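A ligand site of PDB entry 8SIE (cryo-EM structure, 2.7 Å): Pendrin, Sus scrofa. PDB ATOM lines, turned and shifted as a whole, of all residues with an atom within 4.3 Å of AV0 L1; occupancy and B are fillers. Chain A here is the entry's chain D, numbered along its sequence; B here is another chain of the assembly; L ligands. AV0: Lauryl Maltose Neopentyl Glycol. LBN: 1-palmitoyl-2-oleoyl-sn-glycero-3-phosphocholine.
O of Glu 348 sits close to OBX of AV0 L1.
Asn 248 touches AV0 L1 (ND2 to OAJ, 3.8 Å).
CB of Leu 350 touches CBI of AV0 L1, 3.99 Å away.
Thr 351 touches AV0 L1 (CG2 to OAP, 3.4 Å).
Phe 354 touches AV0 L1.
Asp 495 touches AV0 L1.
Leu 496 touches AV0 L1 (CD1 to OAT, 3.8 Å).
Along chain A the residues within 4 Å of AV0 L1 span positions 248 to 496.
An oxygen (O3) of AV0 L1 lies within hydrogen-bond range of the side-chain hydroxyl (OG) of Ser 347, 3.3 Å away.
N of Gly 249 lies close to OAR of AV0 L1.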
ATOM      1  N   SER A 154      -0.264   6.012  23.357  1.00  0.00           N
ATOM      2  CA  SER A 154      -0.156   5.803  21.919  1.00  0.00           C
ATOM      3  C   SER A 154       1.124   6.416  21.358  1.00  0.00           C
ATOM      4  O   SER A 154       1.781   5.822  20.502  1.00  0.00           O
ATOM      5  CB  SER A 154      -1.383   6.365  21.207  1.00  0.00           C
ATOM      6  OG  SER A 154      -1.193   6.397  19.801  1.00  0.00           O
ATOM      7  N   ASN A 248      -3.115   0.257  20.876  1.00  0.00           N
ATOM      8  CA  ASN A 248      -3.615   1.493  20.291  1.00  0.00           C
ATOM      9  C   ASN A 248      -4.381   1.188  19.010  1.00  0.00           C
ATOM     10  O   ASN A 248      -3.972   0.317  18.233  1.00  0.00           O
ATOM     11  CB  ASN A 248      -2.480   2.507  20.075  1.00  0.00           C
ATOM     12  CG  ASN A 248      -1.424   2.042  19.066  1.00  0.00           C
ATOM     13  OD1 ASN A 248      -1.549   1.006  18.417  1.00  0.00           O
ATOM     14  ND2 ASN A 248      -0.361   2.832  18.946  1.00  0.00           N
ATOM     15  N   GLY A 249      -5.521   1.842  18.834  1.00  0.00           N
ATOM     16  CA  GLY A 249      -6.303   1.648  17.636  1.00  0.00           C
ATOM     17  C   GLY A 249      -7.749   1.252  17.886  1.00  0.00           C
ATOM     18  O   GLY A 249      -8.407   1.790  18.772  1.00  0.00           O
ATOM     19  N   SER A 347       0.824  18.307  15.269  1.00  0.00           N
ATOM     20  CA  SER A 347       0.180  17.721  14.099  1.00  0.00           C
ATOM     21  C   SER A 347      -0.375  16.329  14.370  1.00  0.00           C
ATOM     22  O   SER A 347      -1.213  15.848  13.603  1.00  0.00           O
ATOM     23  CB  SER A 347       1.156  17.665  12.932  1.00  0.00           C
ATOM     24  OG  SER A 347       2.245  16.808  13.210  1.00  0.00           O
ATOM     25  N   GLU A 348       0.070  15.669  15.449  1.00  0.00           N
ATOM     26  CA  GLU A 348      -0.377  14.322  15.760  1.00  0.00           C
ATOM     27  C   GLU A 348      -1.402  14.268  16.883  1.00  0.00           C
ATOM     28  O   GLU A 348      -1.757  13.178  17.333  1.00  0.00           O
ATOM     29  CB  GLU A 348       0.824  13.444  16.113  1.00  0.00           C
ATOM     30  CG  GLU A 348       1.890  13.389  15.040  1.00  0.00           C
ATOM     31  CD  GLU A 348       3.215  12.864  15.564  1.00  0.00           C
ATOM     32  OE1 GLU A 348       3.234  11.776  16.172  1.00  0.00           O
ATOM     33  OE2 GLU A 348       4.248  13.538  15.364  1.00  0.00           O
ATOM     34  N   LEU A 350      -4.497  16.485  17.020  1.00  0.00           N
ATOM     35  CA  LEU A 350      -5.584  17.422  16.732  1.00  0.00           C
ATOM     36  C   LEU A 350      -6.945  16.815  17.041  1.00  0.00           C
ATOM     37  O   LEU A 350      -7.739  17.399  17.798  1.00  0.00           O
ATOM     38  CB  LEU A 350      -5.509  17.874  15.278  1.00  0.00           C
ATOM     39  CG  LEU A 350      -4.375  18.866  14.969  1.00  0.00           C
ATOM     40  CD1 LEU A 350      -4.029  18.834  13.487  1.00  0.00           C
ATOM     41  CD2 LEU A 350      -4.754  20.263  15.412  1.00  0.00           C
ATOM     42  N   THR A 351      -7.227  15.634  16.478  1.00  0.00           N
ATOM     43  CA  THR A 351      -8.512  14.981  16.688  1.00  0.00           C
ATOM     44  C   THR A 351      -8.722  14.572  18.142  1.00  0.00           C
ATOM     45  O   THR A 351      -9.859  14.303  18.546  1.00  0.00           O
ATOM     46  CB  THR A 351      -8.647  13.763  15.777  1.00  0.00           C
ATOM     47  OG1 THR A 351     -10.015  13.341  15.729  1.00  0.00           O
ATOM     48  CG2 THR A 351      -7.792  12.623  16.286  1.00  0.00           C
ATOM     49  N   PHE A 354      -9.142  18.354  20.234  1.00  0.00           N
ATOM     50  CA  PHE A 354     -10.466  18.936  20.007  1.00  0.00           C
ATOM     51  C   PHE A 354     -11.505  18.277  20.916  1.00  0.00           C
ATOM     52  O   PHE A 354     -12.267  18.968  21.605  1.00  0.00           O
ATOM     53  CB  PHE A 354     -10.844  18.789  18.535  1.00  0.00           C
ATOM     54  CG  PHE A 354     -12.232  19.280  18.210  1.00  0.00           C
ATOM     55  CD1 PHE A 354     -12.504  20.633  18.133  1.00  0.00           C
ATOM     56  CD2 PHE A 354     -13.254  18.382  17.980  1.00  0.00           C
ATOM     57  CE1 PHE A 354     -13.769  21.079  17.835  1.00  0.00           C
ATOM     58  CE2 PHE A 354     -14.532  18.824  17.688  1.00  0.00           C
ATOM     59  CZ  PHE A 354     -14.780  20.182  17.614  1.00  0.00           C
ATOM     60  N   ASP A 495     -12.175   9.700  21.972  1.00  0.00           N
ATOM     61  CA  ASP A 495     -12.022  10.878  21.129  1.00  0.00           C
ATOM     62  C   ASP A 495     -12.721  10.709  19.789  1.00  0.00           C
ATOM     63  O   ASP A 495     -13.354  11.654  19.294  1.00  0.00           O
ATOM     64  CB  ASP A 495     -10.542  11.196  20.935  1.00  0.00           C
ATOM     65  CG  ASP A 495      -9.779  10.047  20.300  1.00  0.00           C
ATOM     66  OD1 ASP A 495     -10.268   8.901  20.371  1.00  0.00           O
ATOM     67  OD2 ASP A 495      -8.691  10.289  19.749  1.00  0.00           O
ATOM     68  N   LEU A 496     -12.609   9.537  19.176  1.00  0.00           N
ATOM     69  CA  LEU A 496     -13.319   9.287  17.918  1.00  0.00           C
ATOM     70  C   LEU A 496     -14.791   9.009  18.158  1.00  0.00           C
ATOM     71  O   LEU A 496     -15.634   9.358  17.321  1.00  0.00           O
ATOM     72  CB  LEU A 496     -12.663   8.124  17.178  1.00  0.00           C
ATOM     73  CG  LEU A 496     -11.275   8.406  16.584  1.00  0.00           C
ATOM     74  CD1 LEU A 496     -10.778   7.208  15.788  1.00  0.00           C
ATOM     75  CD2 LEU A 496     -11.298   9.657  15.723  1.00  0.00           C
ATOM     76  N   LEU B 499     -16.738  13.794   0.891  1.00  0.00           N
ATOM     77  CA  LEU B 499     -17.266  13.539   2.228  1.00  0.00           C
ATOM     78  C   LEU B 499     -17.343  14.827   3.038  1.00  0.00           C
ATOM     79  O   LEU B 499     -18.326  15.049   3.763  1.00  0.00           O
ATOM     80  CB  LEU B 499     -16.403  12.506   2.944  1.00  0.00           C
ATOM     81  CG  LEU B 499     -16.250  11.157   2.242  1.00  0.00           C
ATOM     82  CD1 LEU B 499     -15.375  10.221   3.054  1.00  0.00           C
ATOM     83  CD2 LEU B 499     -17.613  10.532   1.987  1.00  0.00           C
ATOM     84  N   ALA B 500     -16.328  15.683   2.929  1.00  0.00           N
ATOM     85  CA  ALA B 500     -16.360  16.957   3.630  1.00  0.00           C
ATOM     86  C   ALA B 500     -17.534  17.807   3.155  1.00  0.00           C
ATOM     87  O   ALA B 500     -18.225  18.425   3.971  1.00  0.00           O
ATOM     88  CB  ALA B 500     -15.035  17.701   3.430  1.00  0.00           C
HETATM   89  C1  AV0 L   1      -1.390  13.536   8.980  1.00  0.00           C
HETATM   90  O1  AV0 L   1      -2.765  13.806   8.997  1.00  0.00           O
HETATM   91  C2  AV0 L   1      -0.659  14.779   9.472  1.00  0.00           C
HETATM   92  O2  AV0 L   1      -0.822  15.834   8.534  1.00  0.00           O
HETATM   93  C3  AV0 L   1       0.827  14.501   9.665  1.00  0.00           C
HETATM   94  O3  AV0 L   1       1.456  15.625  10.261  1.00  0.00           O
HETATM   95  C4  AV0 L   1       0.998  13.265  10.525  1.00  0.00           C
HETATM   96  O4  AV0 L   1       2.387  12.962  10.734  1.00  0.00           O
HETATM   97  C5  AV0 L   1       0.270  12.091   9.889  1.00  0.00           C
HETATM   98  O5  AV0 L   1      -1.117  12.415   9.809  1.00  0.00           O
HETATM   99  C6  AV0 L   1       0.375  10.807  10.675  1.00  0.00           C
HETATM  100  O6  AV0 L   1      -0.364   9.758  10.067  1.00  0.00           O
HETATM  101  CAA AV0 L   1     -13.140  21.288  14.304  1.00  0.00           C
HETATM  102  CAB AV0 L   1     -15.567  13.821   6.734  1.00  0.00           C
HETATM  103  OAI AV0 L   1       4.253  16.806  10.098  1.00  0.00           O
HETATM  104  OAJ AV0 L   1      -2.334   4.683  16.290  1.00  0.00           O
HETATM  105  OAL AV0 L   1      -1.340   9.446  13.266  1.00  0.00           O
HETATM  106  OAN AV0 L   1      -6.384   9.483  14.398  1.00  0.00           O
HETATM  107  OAP AV0 L   1      -6.721  11.906  13.161  1.00  0.00           O
HETATM  108  OAQ AV0 L   1       6.300  13.763  12.279  1.00  0.00           O
HETATM  109  OAR AV0 L   1      -6.321   4.855  17.687  1.00  0.00           O
HETATM  110  OAS AV0 L   1       6.028  11.057  11.312  1.00  0.00           O
HETATM  111  OAT AV0 L   1      -7.545   7.529  17.814  1.00  0.00           O
HETATM  112  OAU AV0 L   1       3.538  10.541  10.006  1.00  0.00           O
HETATM  113  OAV AV0 L   1      -4.446   8.786  18.701  1.00  0.00           O
HETATM  114  CAW AV0 L   1     -13.815  20.024  13.833  1.00  0.00           C
HETATM  115  CAX AV0 L   1     -14.231  14.064   6.070  1.00  0.00           C
HETATM  116  CAY AV0 L   1     -13.001  18.778  14.117  1.00  0.00           C
HETATM  117  CAZ AV0 L   1     -13.093  14.189   7.059  1.00  0.00           C
HETATM  118  CBA AV0 L   1     -11.594  18.825  13.565  1.00  0.00           C
HETATM  119  CBB AV0 L   1     -11.735  14.455   6.423  1.00  0.00           C
HETATM  120  CBC AV0 L   1     -10.869  17.493  13.569  1.00  0.00           C
HETATM  121  CBD AV0 L   1     -10.598  14.552   7.427  1.00  0.00           C
HETATM  122  CBE AV0 L   1      -9.459  17.571  12.987  1.00  0.00           C
HETATM  123  CBF AV0 L   1      -9.245  14.856   6.807  1.00  0.00           C
HETATM  124  CBG AV0 L   1      -8.815  16.222  12.705  1.00  0.00           C
HETATM  125  CBH AV0 L   1      -8.129  14.979   7.838  1.00  0.00           C
HETATM  126  CBI AV0 L   1      -7.419  16.345  12.126  1.00  0.00           C
HETATM  127  CBJ AV0 L   1      -6.767  15.305   7.238  1.00  0.00           C
HETATM  128  CBK AV0 L   1      -6.762  15.034  11.737  1.00  0.00           C
HETATM  129  CBL AV0 L   1      -5.659  15.380   8.286  1.00  0.00           C
HETATM  130  CBM AV0 L   1       5.241  15.862  10.450  1.00  0.00           C
HETATM  131  CBN AV0 L   1      -3.757   4.765  16.282  1.00  0.00           C
HETATM  132  CBP AV0 L   1      -2.070  10.668  13.207  1.00  0.00           C
HETATM  133  CBQ AV0 L   1      -5.308  15.231  11.325  1.00  0.00           C
HETATM  134  CBR AV0 L   1      -5.542  14.099   9.103  1.00  0.00           C
HETATM  135  CBS AV0 L   1      -3.273  14.607  10.049  1.00  0.00           C
HETATM  136  CBT AV0 L   1      -4.702  12.802  11.051  1.00  0.00           C
HETATM  137  OBV AV0 L   1      -3.873  12.829  12.200  1.00  0.00           O
HETATM  138  OBX AV0 L   1      -3.411  12.231  14.436  1.00  0.00           O
HETATM  139  OBY AV0 L   1       3.937  14.124   9.505  1.00  0.00           O
HETATM  140  OBZ AV0 L   1      -3.626   7.109  16.595  1.00  0.00           O
HETATM  141  OCB AV0 L   1      -3.848   9.350  16.014  1.00  0.00           O
HETATM  142  CCC AV0 L   1       4.642  14.496  10.695  1.00  0.00           C
HETATM  143  CCD AV0 L   1      -4.236   5.926  17.129  1.00  0.00           C
HETATM  144  CCF AV0 L   1      -2.890  10.880  14.458  1.00  0.00           C
HETATM  145  CCH AV0 L   1      -5.375  10.485  14.526  1.00  0.00           C
HETATM  146  CCJ AV0 L   1      -4.415  12.519  13.465  1.00  0.00           C
HETATM  147  CCL AV0 L   1      -5.410  11.376  13.304  1.00  0.00           C
HETATM  148  CCM AV0 L   1      -4.700  14.173  10.387  1.00  0.00           C
HETATM  149  CCN AV0 L   1       5.688  13.435  11.039  1.00  0.00           C
HETATM  150  CCO AV0 L   1      -5.759   6.053  17.146  1.00  0.00           C
HETATM  151  CCQ AV0 L   1      -3.997   9.854  14.673  1.00  0.00           C
HETATM  152  CCR AV0 L   1       3.244  12.904   9.624  1.00  0.00           C
HETATM  153  CCS AV0 L   1      -4.533   8.182  16.372  1.00  0.00           C
HETATM  154  CCT AV0 L   1       5.038  12.061  11.126  1.00  0.00           C
HETATM  155  CCU AV0 L   1      -6.167   7.253  17.999  1.00  0.00           C
HETATM  156  CCV AV0 L   1       4.233  11.768   9.859  1.00  0.00           C
HETATM  157  CCW AV0 L   1      -5.331   8.468  17.634  1.00  0.00           C
HETATM  158  C1  LBN L   2     -29.952  35.135  13.302  1.00  0.00           C
HETATM  159  P1  LBN L   2     -32.219  35.064  11.984  1.00  0.00           P
HETATM  160  C2  LBN L   2     -28.905  34.211  13.874  1.00  0.00           C
HETATM  161  C3  LBN L   2     -27.736  34.972  14.446  1.00  0.00           C
HETATM  162  C4  LBN L   2     -18.491  37.223  16.730  1.00  0.00           C
HETATM  163  C5  LBN L   2     -21.368  25.697  13.702  1.00  0.00           C
HETATM  164  O1  LBN L   2     -31.015  34.343  12.731  1.00  0.00           O
HETATM  165  C7  LBN L   2     -16.982  37.418  16.713  1.00  0.00           C
HETATM  166  C8  LBN L   2     -20.702  24.654  14.547  1.00  0.00           C
HETATM  167  O2  LBN L   2     -31.512  36.144  11.048  1.00  0.00           O
HETATM  168  C10 LBN L   2     -16.547  38.871  16.652  1.00  0.00           C
HETATM  169  C11 LBN L   2     -19.401  24.151  13.940  1.00  0.00           C
HETATM  170  O3  LBN L   2     -32.849  34.059  11.089  1.00  0.00           O
HETATM  171  C13 LBN L   2     -15.973  39.287  15.297  1.00  0.00           C
HETATM  172  C14 LBN L   2     -18.695  23.100  14.779  1.00  0.00           C
HETATM  173  O4  LBN L   2     -33.056  35.762  12.982  1.00  0.00           O
HETATM  174  C17 LBN L   2     -19.566  21.884  15.083  1.00  0.00           C
HETATM  175  C20 LBN L   2     -18.853  20.824  15.913  1.00  0.00           C
HETATM  176  C22 LBN L   2     -17.612  20.259  15.251  1.00  0.00           C
HETATM  177  C23 LBN L   2     -17.891  19.543  13.937  1.00  0.00           C
HETATM  178  C24 LBN L   2     -18.772  18.338  14.098  1.00  0.00           C
HETATM  179  C25 LBN L   2     -26.779  33.731  16.226  1.00  0.00           C
HETATM  180  O5  LBN L   2     -26.755  34.029  14.929  1.00  0.00           O
HETATM  181  C26 LBN L   2     -25.691  32.765  16.588  1.00  0.00           C
HETATM  182  O6  LBN L   2     -27.572  34.189  17.004  1.00  0.00           O
HETATM  183  C27 LBN L   2     -25.001  33.093  17.912  1.00  0.00           C
HETATM  184  C28 LBN L   2     -24.401  34.493  17.930  1.00  0.00           C
HETATM  185  C29 LBN L   2     -22.881  34.504  18.025  1.00  0.00           C
HETATM  186  C30 LBN L   2     -22.185  33.766  16.898  1.00  0.00           C
HETATM  187  C31 LBN L   2     -20.680  33.980  16.850  1.00  0.00           C
HETATM  188  C32 LBN L   2     -20.280  35.419  16.535  1.00  0.00           C
HETATM  189  C33 LBN L   2     -18.920  35.815  17.093  1.00  0.00           C
HETATM  190  C34 LBN L   2     -27.526  33.804  11.927  1.00  0.00           C
HETATM  191  O7  LBN L   2     -28.434  33.326  12.807  1.00  0.00           O
HETATM  192  C35 LBN L   2     -26.262  32.992  11.958  1.00  0.00           C
HETATM  193  O8  LBN L   2     -27.726  34.733  11.197  1.00  0.00           O
HETATM  194  C36 LBN L   2     -26.396  31.710  12.772  1.00  0.00           C
HETATM  195  C37 LBN L   2     -25.055  31.151  13.217  1.00  0.00           C
HETATM  196  C38 LBN L   2     -24.091  30.889  12.074  1.00  0.00           C
HETATM  197  C39 LBN L   2     -22.780  30.235  12.509  1.00  0.00           C
HETATM  198  C40 LBN L   2     -22.965  28.890  13.195  1.00  0.00           C
HETATM  199  C41 LBN L   2     -21.658  28.185  13.531  1.00  0.00           C
HETATM  200  C42 LBN L   2     -21.870  26.834  14.134  1.00  0.00           C
